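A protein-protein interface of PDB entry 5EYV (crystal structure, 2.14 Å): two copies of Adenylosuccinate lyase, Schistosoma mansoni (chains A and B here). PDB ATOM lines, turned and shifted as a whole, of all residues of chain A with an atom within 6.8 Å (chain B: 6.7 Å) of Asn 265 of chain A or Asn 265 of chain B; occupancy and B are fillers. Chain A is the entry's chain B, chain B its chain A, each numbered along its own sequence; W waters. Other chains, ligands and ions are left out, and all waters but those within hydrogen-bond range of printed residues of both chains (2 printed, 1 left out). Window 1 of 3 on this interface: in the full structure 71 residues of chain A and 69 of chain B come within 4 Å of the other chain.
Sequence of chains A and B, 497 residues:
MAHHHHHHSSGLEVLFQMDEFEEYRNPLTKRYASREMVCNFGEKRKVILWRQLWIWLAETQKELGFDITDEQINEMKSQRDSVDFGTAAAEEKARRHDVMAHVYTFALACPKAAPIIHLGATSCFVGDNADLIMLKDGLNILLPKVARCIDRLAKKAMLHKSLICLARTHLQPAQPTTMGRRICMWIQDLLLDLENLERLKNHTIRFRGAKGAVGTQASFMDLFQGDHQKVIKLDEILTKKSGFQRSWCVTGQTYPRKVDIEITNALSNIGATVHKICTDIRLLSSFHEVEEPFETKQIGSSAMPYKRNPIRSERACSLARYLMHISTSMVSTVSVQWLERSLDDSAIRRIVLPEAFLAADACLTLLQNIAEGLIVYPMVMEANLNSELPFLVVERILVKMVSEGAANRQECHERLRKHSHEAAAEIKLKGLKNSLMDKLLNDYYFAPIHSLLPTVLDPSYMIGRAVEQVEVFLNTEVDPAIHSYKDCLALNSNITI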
ATOM      1  N   LEU A 200      -4.424 -18.871 -26.168  1.00  0.00           N
ATOM      2  CA  LEU A 200      -4.259 -18.874 -24.716  1.00  0.00           C
ATOM      3  C   LEU A 200      -4.631 -20.226 -24.122  1.00  0.00           C
ATOM      4  O   LEU A 200      -3.892 -20.788 -23.305  1.00  0.00           O
ATOM      5  CB  LEU A 200      -5.115 -17.773 -24.091  1.00  0.00           C
ATOM      6  CG  LEU A 200      -4.463 -16.433 -23.762  1.00  0.00           C
ATOM      7  CD1 LEU A 200      -5.505 -15.482 -23.197  1.00  0.00           C
ATOM      8  CD2 LEU A 200      -3.324 -16.627 -22.777  1.00  0.00           C
ATOM      9  N   VAL A 259       2.186 -15.191 -17.795  1.00  0.00           N
ATOM     10  CA  VAL A 259       0.947 -15.792 -18.281  1.00  0.00           C
ATOM     11  C   VAL A 259      -0.249 -14.943 -17.872  1.00  0.00           C
ATOM     12  O   VAL A 259      -1.220 -14.807 -18.626  1.00  0.00           O
ATOM     13  CB  VAL A 259       0.826 -17.240 -17.770  1.00  0.00           C
ATOM     14  CG1 VAL A 259      -0.537 -17.823 -18.119  1.00  0.00           C
ATOM     15  CG2 VAL A 259       1.936 -18.089 -18.354  1.00  0.00           C
ATOM     16  N   ASP A 260      -0.196 -14.349 -16.677  1.00  0.00           N
ATOM     17  CA  ASP A 260      -1.276 -13.467 -16.248  1.00  0.00           C
ATOM     18  C   ASP A 260      -1.338 -12.204 -17.096  1.00  0.00           C
ATOM     19  O   ASP A 260      -2.433 -11.687 -17.354  1.00  0.00           O
ATOM     20  CB  ASP A 260      -1.121 -13.113 -14.769  1.00  0.00           C
ATOM     21  CG  ASP A 260      -1.341 -14.306 -13.858  1.00  0.00           C
ATOM     22  OD1 ASP A 260      -2.030 -15.257 -14.284  1.00  0.00           O
ATOM     23  OD2 ASP A 260      -0.829 -14.293 -12.720  1.00  0.00           O
ATOM     24  N   ILE A 261      -0.185 -11.693 -17.537  1.00  0.00           N
ATOM     25  CA  ILE A 261      -0.181 -10.591 -18.495  1.00  0.00           C
ATOM     26  C   ILE A 261      -0.829 -11.029 -19.799  1.00  0.00           C
ATOM     27  O   ILE A 261      -1.700 -10.340 -20.343  1.00  0.00           O
ATOM     28  CB  ILE A 261       1.251 -10.083 -18.738  1.00  0.00           C
ATOM     29  CG1 ILE A 261       1.844  -9.466 -17.474  1.00  0.00           C
ATOM     30  CG2 ILE A 261       1.265  -9.070 -19.876  1.00  0.00           C
ATOM     31  CD1 ILE A 261       3.255  -8.946 -17.687  1.00  0.00           C
ATOM     32  N   GLU A 262      -0.400 -12.181 -20.322  1.00  0.00           N
ATOM     33  CA  GLU A 262      -0.948 -12.701 -21.572  1.00  0.00           C
ATOM     34  C   GLU A 262      -2.463 -12.829 -21.499  1.00  0.00           C
ATOM     35  O   GLU A 262      -3.177 -12.448 -22.433  1.00  0.00           O
ATOM     36  CB  GLU A 262      -0.317 -14.058 -21.892  1.00  0.00           C
ATOM     37  CG  GLU A 262       1.189 -14.029 -22.086  1.00  0.00           C
ATOM     38  CD  GLU A 262       1.589 -13.554 -23.465  1.00  0.00           C
ATOM     39  OE1 GLU A 262       0.701 -13.447 -24.337  1.00  0.00           O
ATOM     40  OE2 GLU A 262       2.792 -13.292 -23.679  1.00  0.00           O
ATOM     41  N   ILE A 263      -2.969 -13.361 -20.385  1.00  0.00           N
ATOM     42  CA  ILE A 263      -4.407 -13.571 -20.242  1.00  0.00           C
ATOM     43  C   ILE A 263      -5.141 -12.236 -20.216  1.00  0.00           C
ATOM     44  O   ILE A 263      -6.087 -12.013 -20.981  1.00  0.00           O
ATOM     45  CB  ILE A 263      -4.704 -14.403 -18.982  1.00  0.00           C
ATOM     46  CG1 ILE A 263      -4.178 -15.831 -19.149  1.00  0.00           C
ATOM     47  CG2 ILE A 263      -6.197 -14.413 -18.689  1.00  0.00           C
ATOM     48  CD1 ILE A 263      -4.369 -16.697 -17.923  1.00  0.00           C
ATOM     49  N   THR A 264      -4.712 -11.325 -19.338  1.00  0.00           N
ATOM     50  CA  THR A 264      -5.417 -10.055 -19.203  1.00  0.00           C
ATOM     51  C   THR A 264      -5.210  -9.156 -20.419  1.00  0.00           C
ATOM     52  O   THR A 264      -6.079  -8.333 -20.729  1.00  0.00           O
ATOM     53  CB  THR A 264      -4.985  -9.343 -17.918  1.00  0.00           C
ATOM     54  OG1 THR A 264      -3.562  -9.174 -17.909  1.00  0.00           O
ATOM     55  CG2 THR A 264      -5.400 -10.155 -16.696  1.00  0.00           C
ATOM     56  N   ASN A 265      -4.082  -9.298 -21.121  1.00  0.00           N
ATOM     57  CA  ASN A 265      -3.882  -8.545 -22.357  1.00  0.00           C
ATOM     58  C   ASN A 265      -4.926  -8.913 -23.404  1.00  0.00           C
ATOM     59  O   ASN A 265      -5.486  -8.033 -24.071  1.00  0.00           O
ATOM     60  CB  ASN A 265      -2.477  -8.786 -22.910  1.00  0.00           C
ATOM     61  CG  ASN A 265      -1.464  -7.777 -22.405  1.00  0.00           C
ATOM     62  OD1 ASN A 265      -1.794  -6.882 -21.628  1.00  0.00           O
ATOM     63  ND2 ASN A 265      -0.219  -7.922 -22.844  1.00  0.00           N
ATOM     64  N   ALA A 266      -5.196 -10.210 -23.568  1.00  0.00           N
ATOM     65  CA  ALA A 266      -6.189 -10.637 -24.547  1.00  0.00           C
ATOM     66  C   ALA A 266      -7.595 -10.245 -24.114  1.00  0.00           C
ATOM     67  O   ALA A 266      -8.427  -9.873 -24.950  1.00  0.00           O
ATOM     68  CB  ALA A 266      -6.097 -12.145 -24.771  1.00  0.00           C
ATOM     69  N   LEU A 267      -7.880 -10.321 -22.812  1.00  0.00           N
ATOM     70  CA  LEU A 267      -9.191  -9.900 -22.328  1.00  0.00           C
ATOM     71  C   LEU A 267      -9.381  -8.400 -22.500  1.00  0.00           C
ATOM     72  O   LEU A 267     -10.460  -7.949 -22.902  1.00  0.00           O
ATOM     73  CB  LEU A 267      -9.373 -10.307 -20.867  1.00  0.00           C
ATOM     74  CG  LEU A 267      -9.327 -11.812 -20.591  1.00  0.00           C
ATOM     75  CD1 LEU A 267      -9.796 -12.119 -19.176  1.00  0.00           C
ATOM     76  CD2 LEU A 267     -10.150 -12.579 -21.617  1.00  0.00           C
ATOM     77  N   SER A 268      -8.342  -7.609 -22.214  1.00  0.00           N
ATOM     78  CA  SER A 268      -8.411  -6.176 -22.477  1.00  0.00           C
ATOM     79  C   SER A 268      -8.622  -5.891 -23.958  1.00  0.00           C
ATOM     80  O   SER A 268      -9.257  -4.892 -24.312  1.00  0.00           O
ATOM     81  CB  SER A 268      -7.142  -5.481 -21.982  1.00  0.00           C
ATOM     82  OG  SER A 268      -7.118  -5.397 -20.567  1.00  0.00           O
ATOM     83  N   ASN A 269      -8.093  -6.752 -24.833  1.00  0.00           N
ATOM     84  CA  ASN A 269      -8.325  -6.588 -26.263  1.00  0.00           C
ATOM     85  C   ASN A 269      -9.792  -6.775 -26.616  1.00  0.00           C
ATOM     86  O   ASN A 269     -10.291  -6.138 -27.551  1.00  0.00           O
ATOM     87  CB  ASN A 269      -7.464  -7.570 -27.056  1.00  0.00           C
ATOM     88  CG  ASN A 269      -6.255  -6.910 -27.680  1.00  0.00           C
ATOM     89  OD1 ASN A 269      -5.158  -6.940 -27.121  1.00  0.00           O
ATOM     90  ND2 ASN A 269      -6.449  -6.304 -28.846  1.00  0.00           N
ATOM     91  N   ILE A 270     -10.496  -7.650 -25.893  1.00  0.00           N
ATOM     92  CA  ILE A 270     -11.932  -7.808 -26.100  1.00  0.00           C
ATOM     93  C   ILE A 270     -12.656  -6.503 -25.798  1.00  0.00           C
ATOM     94  O   ILE A 270     -13.564  -6.095 -26.531  1.00  0.00           O
ATOM     95  CB  ILE A 270     -12.482  -8.957 -25.234  1.00  0.00           C
ATOM     96  CG1 ILE A 270     -11.626 -10.217 -25.385  1.00  0.00           C
ATOM     97  CG2 ILE A 270     -13.937  -9.239 -25.588  1.00  0.00           C
ATOM     98  CD1 ILE A 270     -11.835 -10.954 -26.677  1.00  0.00           C
ATOM     99  N   MET A 324     -10.697  -2.719 -20.400  1.00  0.00           N
ATOM    100  CA  MET A 324      -9.590  -2.260 -21.234  1.00  0.00           C
ATOM    101  C   MET A 324      -8.326  -2.021 -20.420  1.00  0.00           C
ATOM    102  O   MET A 324      -7.218  -2.327 -20.876  1.00  0.00           O
ATOM    103  CB  MET A 324      -9.987  -0.979 -21.967  1.00  0.00           C
ATOM    104  CG  MET A 324     -10.475  -1.179 -23.383  1.00  0.00           C
ATOM    105  SD  MET A 324     -11.211   0.337 -24.013  1.00  0.00           S
ATOM    106  CE  MET A 324      -9.944   1.532 -23.597  1.00  0.00           C
ATOM    107  N   SER A 327      -5.468  -4.811 -17.204  1.00  0.00           N
ATOM    108  CA  SER A 327      -4.209  -5.536 -17.309  1.00  0.00           C
ATOM    109  C   SER A 327      -3.010  -4.725 -16.833  1.00  0.00           C
ATOM    110  O   SER A 327      -1.936  -5.305 -16.635  1.00  0.00           O
ATOM    111  CB  SER A 327      -3.980  -5.984 -18.754  1.00  0.00           C
ATOM    112  OG  SER A 327      -3.844  -4.869 -19.618  1.00  0.00           O
ATOM    113  N   THR A 328      -3.162  -3.413 -16.639  1.00  0.00           N
ATOM    114  CA  THR A 328      -2.017  -2.574 -16.300  1.00  0.00           C
ATOM    115  C   THR A 328      -1.448  -2.881 -14.920  1.00  0.00           C
ATOM    116  O   THR A 328      -0.295  -2.532 -14.651  1.00  0.00           O
ATOM    117  CB  THR A 328      -2.400  -1.094 -16.383  1.00  0.00           C
ATOM    118  OG1 THR A 328      -1.226  -0.288 -16.227  1.00  0.00           O
ATOM    119  CG2 THR A 328      -3.388  -0.737 -15.294  1.00  0.00           C
ATOM    120  N   VAL A 331       0.967  -6.224 -15.459  1.00  0.00           N
ATOM    121  CA  VAL A 331       2.306  -5.949 -15.967  1.00  0.00           C
ATOM    122  C   VAL A 331       3.183  -5.365 -14.864  1.00  0.00           C
ATOM    123  O   VAL A 331       4.379  -5.669 -14.779  1.00  0.00           O
ATOM    124  CB  VAL A 331       2.242  -5.034 -17.207  1.00  0.00           C
ATOM    125  CG1 VAL A 331       1.445  -3.778 -16.921  1.00  0.00           C
ATOM    126  CG2 VAL A 331       3.644  -4.681 -17.689  1.00  0.00           C
ATOM    127  N   ASN B 196       6.381 -14.404 -28.878  1.00  0.00           N
ATOM    128  CA  ASN B 196       5.391 -13.381 -29.204  1.00  0.00           C
ATOM    129  C   ASN B 196       5.865 -12.485 -30.341  1.00  0.00           C
ATOM    130  O   ASN B 196       5.090 -12.158 -31.247  1.00  0.00           O
ATOM    131  CB  ASN B 196       5.070 -12.541 -27.966  1.00  0.00           C
ATOM    132  CG  ASN B 196       4.294 -13.314 -26.920  1.00  0.00           C
ATOM    133  OD1 ASN B 196       3.747 -14.381 -27.199  1.00  0.00           O
ATOM    134  ND2 ASN B 196       4.231 -12.770 -25.710  1.00  0.00           N
ATOM    135  N   LEU B 200       4.191 -11.953 -34.120  1.00  0.00           N
ATOM    136  CA  LEU B 200       3.838 -10.636 -34.644  1.00  0.00           C
ATOM    137  C   LEU B 200       4.400 -10.436 -36.043  1.00  0.00           C
ATOM    138  O   LEU B 200       3.704  -9.949 -36.943  1.00  0.00           O
ATOM    139  CB  LEU B 200       4.356  -9.545 -33.709  1.00  0.00           C
ATOM    140  CG  LEU B 200       3.486  -9.099 -32.536  1.00  0.00           C
ATOM    141  CD1 LEU B 200       4.245  -8.082 -31.708  1.00  0.00           C
ATOM    142  CD2 LEU B 200       2.180  -8.511 -33.036  1.00  0.00           C
ATOM    143  N   ASP B 260      -1.885  -2.515 -33.704  1.00  0.00           N
ATOM    144  CA  ASP B 260      -1.001  -1.688 -32.887  1.00  0.00           C
ATOM    145  C   ASP B 260      -1.072  -2.069 -31.414  1.00  0.00           C
ATOM    146  O   ASP B 260      -0.081  -1.917 -30.690  1.00  0.00           O
ATOM    147  CB  ASP B 260      -1.340  -0.208 -33.070  1.00  0.00           C
ATOM    148  CG  ASP B 260      -1.001   0.301 -34.460  1.00  0.00           C
ATOM    149  OD1 ASP B 260      -0.208  -0.362 -35.163  1.00  0.00           O
ATOM    150  OD2 ASP B 260      -1.524   1.367 -34.847  1.00  0.00           O
ATOM    151  N   ILE B 261      -2.224  -2.558 -30.950  1.00  0.00           N
ATOM    152  CA  ILE B 261      -2.308  -3.069 -29.585  1.00  0.00           C
ATOM    153  C   ILE B 261      -1.413  -4.291 -29.428  1.00  0.00           C
ATOM    154  O   ILE B 261      -0.633  -4.395 -28.474  1.00  0.00           O
ATOM    155  CB  ILE B 261      -3.766  -3.391 -29.212  1.00  0.00           C
ATOM    156  CG1 ILE B 261      -4.604  -2.116 -29.153  1.00  0.00           C
ATOM    157  CG2 ILE B 261      -3.820  -4.120 -27.878  1.00  0.00           C
ATOM    158  CD1 ILE B 261      -6.039  -2.358 -28.733  1.00  0.00           C
ATOM    159  N   GLU B 262      -1.511  -5.232 -30.371  1.00  0.00           N
ATOM    160  CA  GLU B 262      -0.709  -6.451 -30.301  1.00  0.00           C
ATOM    161  C   GLU B 262       0.780  -6.134 -30.268  1.00  0.00           C
ATOM    162  O   GLU B 262       1.545  -6.781 -29.543  1.00  0.00           O
ATOM    163  CB  GLU B 262      -1.033  -7.356 -31.491  1.00  0.00           C
ATOM    164  CG  GLU B 262      -2.518  -7.596 -31.703  1.00  0.00           C
ATOM    165  CD  GLU B 262      -3.131  -8.458 -30.618  1.00  0.00           C
ATOM    166  OE1 GLU B 262      -2.496  -9.459 -30.222  1.00  0.00           O
ATOM    167  OE2 GLU B 262      -4.246  -8.133 -30.157  1.00  0.00           O
ATOM    168  N   ILE B 263       1.208  -5.136 -31.041  1.00  0.00           N
ATOM    169  CA  ILE B 263       2.622  -4.781 -31.092  1.00  0.00           C
ATOM    170  C   ILE B 263       3.079  -4.209 -29.755  1.00  0.00           C
ATOM    171  O   ILE B 263       4.047  -4.690 -29.156  1.00  0.00           O
ATOM    172  CB  ILE B 263       2.882  -3.801 -32.250  1.00  0.00           C
ATOM    173  CG1 ILE B 263       2.608  -4.486 -33.591  1.00  0.00           C
ATOM    174  CG2 ILE B 263       4.306  -3.268 -32.193  1.00  0.00           C
ATOM    175  CD1 ILE B 263       2.818  -3.588 -34.791  1.00  0.00           C
ATOM    176  N   THR B 264       2.385  -3.178 -29.264  1.00  0.00           N
ATOM    177  CA  THR B 264       2.807  -2.529 -28.026  1.00  0.00           C
ATOM    178  C   THR B 264       2.634  -3.443 -26.817  1.00  0.00           C
ATOM    179  O   THR B 264       3.432  -3.373 -25.876  1.00  0.00           O
ATOM    180  CB  THR B 264       2.038  -1.221 -27.821  1.00  0.00           C
ATOM    181  OG1 THR B 264       0.626  -1.477 -27.848  1.00  0.00           O
ATOM    182  CG2 THR B 264       2.390  -0.217 -28.913  1.00  0.00           C
ATOM    183  N   ASN B 265       1.606  -4.298 -26.819  1.00  0.00           N
ATOM    184  CA  ASN B 265       1.445  -5.261 -25.732  1.00  0.00           C
ATOM    185  C   ASN B 265       2.651  -6.184 -25.630  1.00  0.00           C
ATOM    186  O   ASN B 265       3.145  -6.453 -24.527  1.00  0.00           O
ATOM    187  CB  ASN B 265       0.169  -6.083 -25.930  1.00  0.00           C
ATOM    188  CG  ASN B 265      -1.072  -5.368 -25.433  1.00  0.00           C
ATOM    189  OD1 ASN B 265      -1.004  -4.233 -24.958  1.00  0.00           O
ATOM    190  ND2 ASN B 265      -2.218  -6.029 -25.544  1.00  0.00           N
ATOM    191  N   ALA B 266       3.137  -6.684 -26.769  1.00  0.00           N
ATOM    192  CA  ALA B 266       4.309  -7.553 -26.752  1.00  0.00           C
ATOM    193  C   ALA B 266       5.559  -6.785 -26.344  1.00  0.00           C
ATOM    194  O   ALA B 266       6.412  -7.315 -25.624  1.00  0.00           O
ATOM    195  CB  ALA B 266       4.501  -8.204 -28.119  1.00  0.00           C
ATOM    196  N   LEU B 267       5.686  -5.536 -26.797  1.00  0.00           N
ATOM    197  CA  LEU B 267       6.820  -4.718 -26.382  1.00  0.00           C
ATOM    198  C   LEU B 267       6.744  -4.390 -24.896  1.00  0.00           C
ATOM    199  O   LEU B 267       7.757  -4.454 -24.190  1.00  0.00           O
ATOM    200  CB  LEU B 267       6.883  -3.441 -27.218  1.00  0.00           C
ATOM    201  CG  LEU B 267       7.118  -3.637 -28.719  1.00  0.00           C
ATOM    202  CD1 LEU B 267       7.284  -2.298 -29.428  1.00  0.00           C
ATOM    203  CD2 LEU B 267       8.323  -4.536 -28.961  1.00  0.00           C
ATOM    204  N   SER B 268       5.553  -4.044 -24.402  1.00  0.00           N
ATOM    205  CA  SER B 268       5.389  -3.809 -22.970  1.00  0.00           C
ATOM    206  C   SER B 268       5.670  -5.069 -22.165  1.00  0.00           C
ATOM    207  O   SER B 268       6.163  -4.986 -21.034  1.00  0.00           O
ATOM    208  CB  SER B 268       3.981  -3.296 -22.674  1.00  0.00           C
ATOM    209  OG  SER B 268       3.789  -1.995 -23.203  1.00  0.00           O
ATOM    210  N   ASN B 269       5.365  -6.241 -22.726  1.00  0.00           N
ATOM    211  CA  ASN B 269       5.683  -7.497 -22.054  1.00  0.00           C
ATOM    212  C   ASN B 269       7.189  -7.670 -21.908  1.00  0.00           C
ATOM    213  O   ASN B 269       7.666  -8.181 -20.888  1.00  0.00           O
ATOM    214  CB  ASN B 269       5.076  -8.673 -22.825  1.00  0.00           C
ATOM    215  CG  ASN B 269       4.517  -9.739 -21.912  1.00  0.00           C
ATOM    216  OD1 ASN B 269       4.932  -9.865 -20.757  1.00  0.00           O
ATOM    217  ND2 ASN B 269       3.571 -10.514 -22.421  1.00  0.00           N
ATOM    218  N   ILE B 270       7.952  -7.264 -22.926  1.00  0.00           N
ATOM    219  CA  ILE B 270       9.408  -7.280 -22.821  1.00  0.00           C
ATOM    220  C   ILE B 270       9.866  -6.372 -21.690  1.00  0.00           C
ATOM    221  O   ILE B 270      10.790  -6.707 -20.938  1.00  0.00           O
ATOM    222  CB  ILE B 270      10.046  -6.875 -24.163  1.00  0.00           C
ATOM    223  CG1 ILE B 270       9.831  -7.967 -25.211  1.00  0.00           C
ATOM    224  CG2 ILE B 270      11.532  -6.583 -23.989  1.00  0.00           C
ATOM    225  CD1 ILE B 270      10.467  -7.651 -26.544  1.00  0.00           C
ATOM    226  N   SER B 327       1.641   1.056 -23.489  1.00  0.00           N
ATOM    227  CA  SER B 327       0.647   0.326 -24.267  1.00  0.00           C
ATOM    228  C   SER B 327      -0.770   0.836 -24.028  1.00  0.00           C
ATOM    229  O   SER B 327      -1.630   0.678 -24.902  1.00  0.00           O
ATOM    230  CB  SER B 327       0.725  -1.168 -23.942  1.00  0.00           C
ATOM    231  OG  SER B 327      -0.126  -1.921 -24.786  1.00  0.00           O
ATOM    232  N   THR B 328      -1.034   1.444 -22.869  1.00  0.00           N
ATOM    233  CA  THR B 328      -2.389   1.887 -22.555  1.00  0.00           C
ATOM    234  C   THR B 328      -2.872   2.992 -23.485  1.00  0.00           C
ATOM    235  O   THR B 328      -4.085   3.191 -23.613  1.00  0.00           O
ATOM    236  CB  THR B 328      -2.474   2.360 -21.103  1.00  0.00           C
ATOM    237  OG1 THR B 328      -1.402   3.270 -20.828  1.00  0.00           O
ATOM    238  CG2 THR B 328      -2.389   1.175 -20.150  1.00  0.00           C
ATOM    239  N   MET B 330      -2.497   2.971 -26.756  1.00  0.00           N
ATOM    240  CA  MET B 330      -3.000   2.358 -27.982  1.00  0.00           C
ATOM    241  C   MET B 330      -4.368   1.722 -27.766  1.00  0.00           C
ATOM    242  O   MET B 330      -5.241   1.812 -28.636  1.00  0.00           O
ATOM    243  CB  MET B 330      -1.999   1.325 -28.503  1.00  0.00           C
ATOM    244  CG  MET B 330      -0.687   1.916 -29.004  1.00  0.00           C
ATOM    245  SD  MET B 330      -0.855   2.876 -30.525  1.00  0.00           S
ATOM    246  CE  MET B 330      -0.887   4.551 -29.884  1.00  0.00           C
ATOM    247  N   VAL B 331      -4.574   1.073 -26.617  1.00  0.00           N
ATOM    248  CA  VAL B 331      -5.861   0.431 -26.366  1.00  0.00           C
ATOM    249  C   VAL B 331      -6.963   1.473 -26.205  1.00  0.00           C
ATOM    250  O   VAL B 331      -8.115   1.234 -26.589  1.00  0.00           O
ATOM    251  CB  VAL B 331      -5.766  -0.507 -25.146  1.00  0.00           C
ATOM    252  CG1 VAL B 331      -5.363   0.260 -23.900  1.00  0.00           C
ATOM    253  CG2 VAL B 331      -7.078  -1.248 -24.926  1.00  0.00           C
HETATM  254  O   HOH W   1      -3.253  -4.081 -22.570  1.00  0.00           O
HETATM  255  O   HOH W   2      -5.183  -5.463 -24.876  1.00  0.00           O
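ND2 of Asn 196 of chain B is in hydrogen-bond range of OE2 of Glu 262 of chain A. The side-chain amide nitrogen (ND2) of Asn 269 of chain A is in hydrogen-bond range of the side-chain carboxylate (OE2) of Glu 262 of chain B (3.1 Å). OD1 of Asn 269 of chain A sits at hydrogen-bond distance from ND2 of Asn 265 of chain B (3.5 Å). The side-chain carboxylate (OE2) of Glu 262 of chain A lies within hydrogen-bond range of the side-chain amide nitrogen (ND2) of Asn 269 of chain B, at 3.1 Å.
The backbone carbonyl oxygen (O) of Ile 261 of chain B lies within hydrogen-bond range of the side-chain hydroxyl (OG1) of Thr 264 of chain B, 3.2 Å away. The side-chain amide oxygen of Asn 265 of chain B is in hydrogen-bond range of the side-chain hydroxyl of Ser 327 of chain B. The backbone carbonyl oxygen (O) of Ile 261 of chain A lies within hydrogen-bond range of the side-chain hydroxyl (OG1) of Thr 264 of chain A (3.3 Å). O of Asn 265 of chain A lies close to OD1 of Asn 269 of chain A (3.3 Å). O of Met 324 of chain A is in hydrogen-bond range of OG of Ser 268 of chain A.
Among the printed residues, pairs that only touch across the chains: Asn 269 of chain A with Ile 261 of chain B (3.2 Å), Met 324 of chain A with Val 331 of chain B (3.5 Å), Asn 265 of chain A with Asn 265 of chain B (3.6 Å) and Ile 261 of chain A with Asn 269 of chain B (3.6 Å).
Printed residues of chain B within 4 Å of Ile 261 of chain A: Asn 269 (3.6 Å). Of chain B, only Asn 265 comes within 4 Å of Asn 265 of chain A. Of the printed residues of chain B, Met 324 of chain A touches Val 331 (3.5 Å). Of chain A, only Asn 265 (3.6 Å) and Asn 269 (3.5 Å) come within 4 Å of Asn 265 of chain B. The nearest residue of chain A that does not touch Asn 265 of chain B is Ala 266 of chain A (5.5 Å). The nearest printed residue of chain B that does not touch Met 324 of chain A is Thr 328 of chain B (6.0 Å).
Hydrophobic or aromatic side chains of chain B that line the printed part of chain A: Ile 261 and Val 331. Printed residues of chain A that touch a printed residue of chain B: Ile 261, Glu 262, Asn 265, Asn 269 and Met 324. Hydrophobic or aromatic side chains of chain A that line the printed part of chain B: Ile 261 and Met 324. Along chain A the printed residues that touch a printed residue of chain B span positions 261 to 324. Among the printed residues, 8 pairs touch across the chains.
Ile 261 of chain A touches Asn 269 of chain B, and with the chains exchanged Asn 269 of chain A touches Ile 261 of chain B. Glu 262 of chain A touches Asn 269 of chain B, and with the chains exchanged Asn 269 of chain A touches Glu 262 of chain B. Asn 265 of chain A touches its own counterpart, Asn 265 of chain B. Asn 269 of chain A touches Asn 265 of chain B, but with the chains exchanged Asn 265 of chain A does not touch Asn 269 of chain B (4.6 Å). Positions printed for both chains: 200, 260, 261, 262, 263, 264, 265, 266, 267, 268, 269, 270, 327, 328 and 331. Of the 8 pairs that touch across the chains among the printed residues, 5 have their exchanged pair printed and touching as well.
Water W2 lies within hydrogen-bond range of the side-chain amide oxygen (OD1) of Asn 269 of chain A (2.7 Å), the backbone carbonyl oxygen (O) of Asn 265 of chain A (2.7 Å) and the side-chain amide nitrogen (ND2) of Asn 265 of chain B (3.1 Å). Water W1 lies within hydrogen-bond range of the side-chain hydroxyl of Ser 327 of chain A (3.1 Å), the side-chain amide oxygen of Asn 265 of chain B (3.3 Å) and the side-chain amide oxygen of Asn 265 of chain A (3.3 Å).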
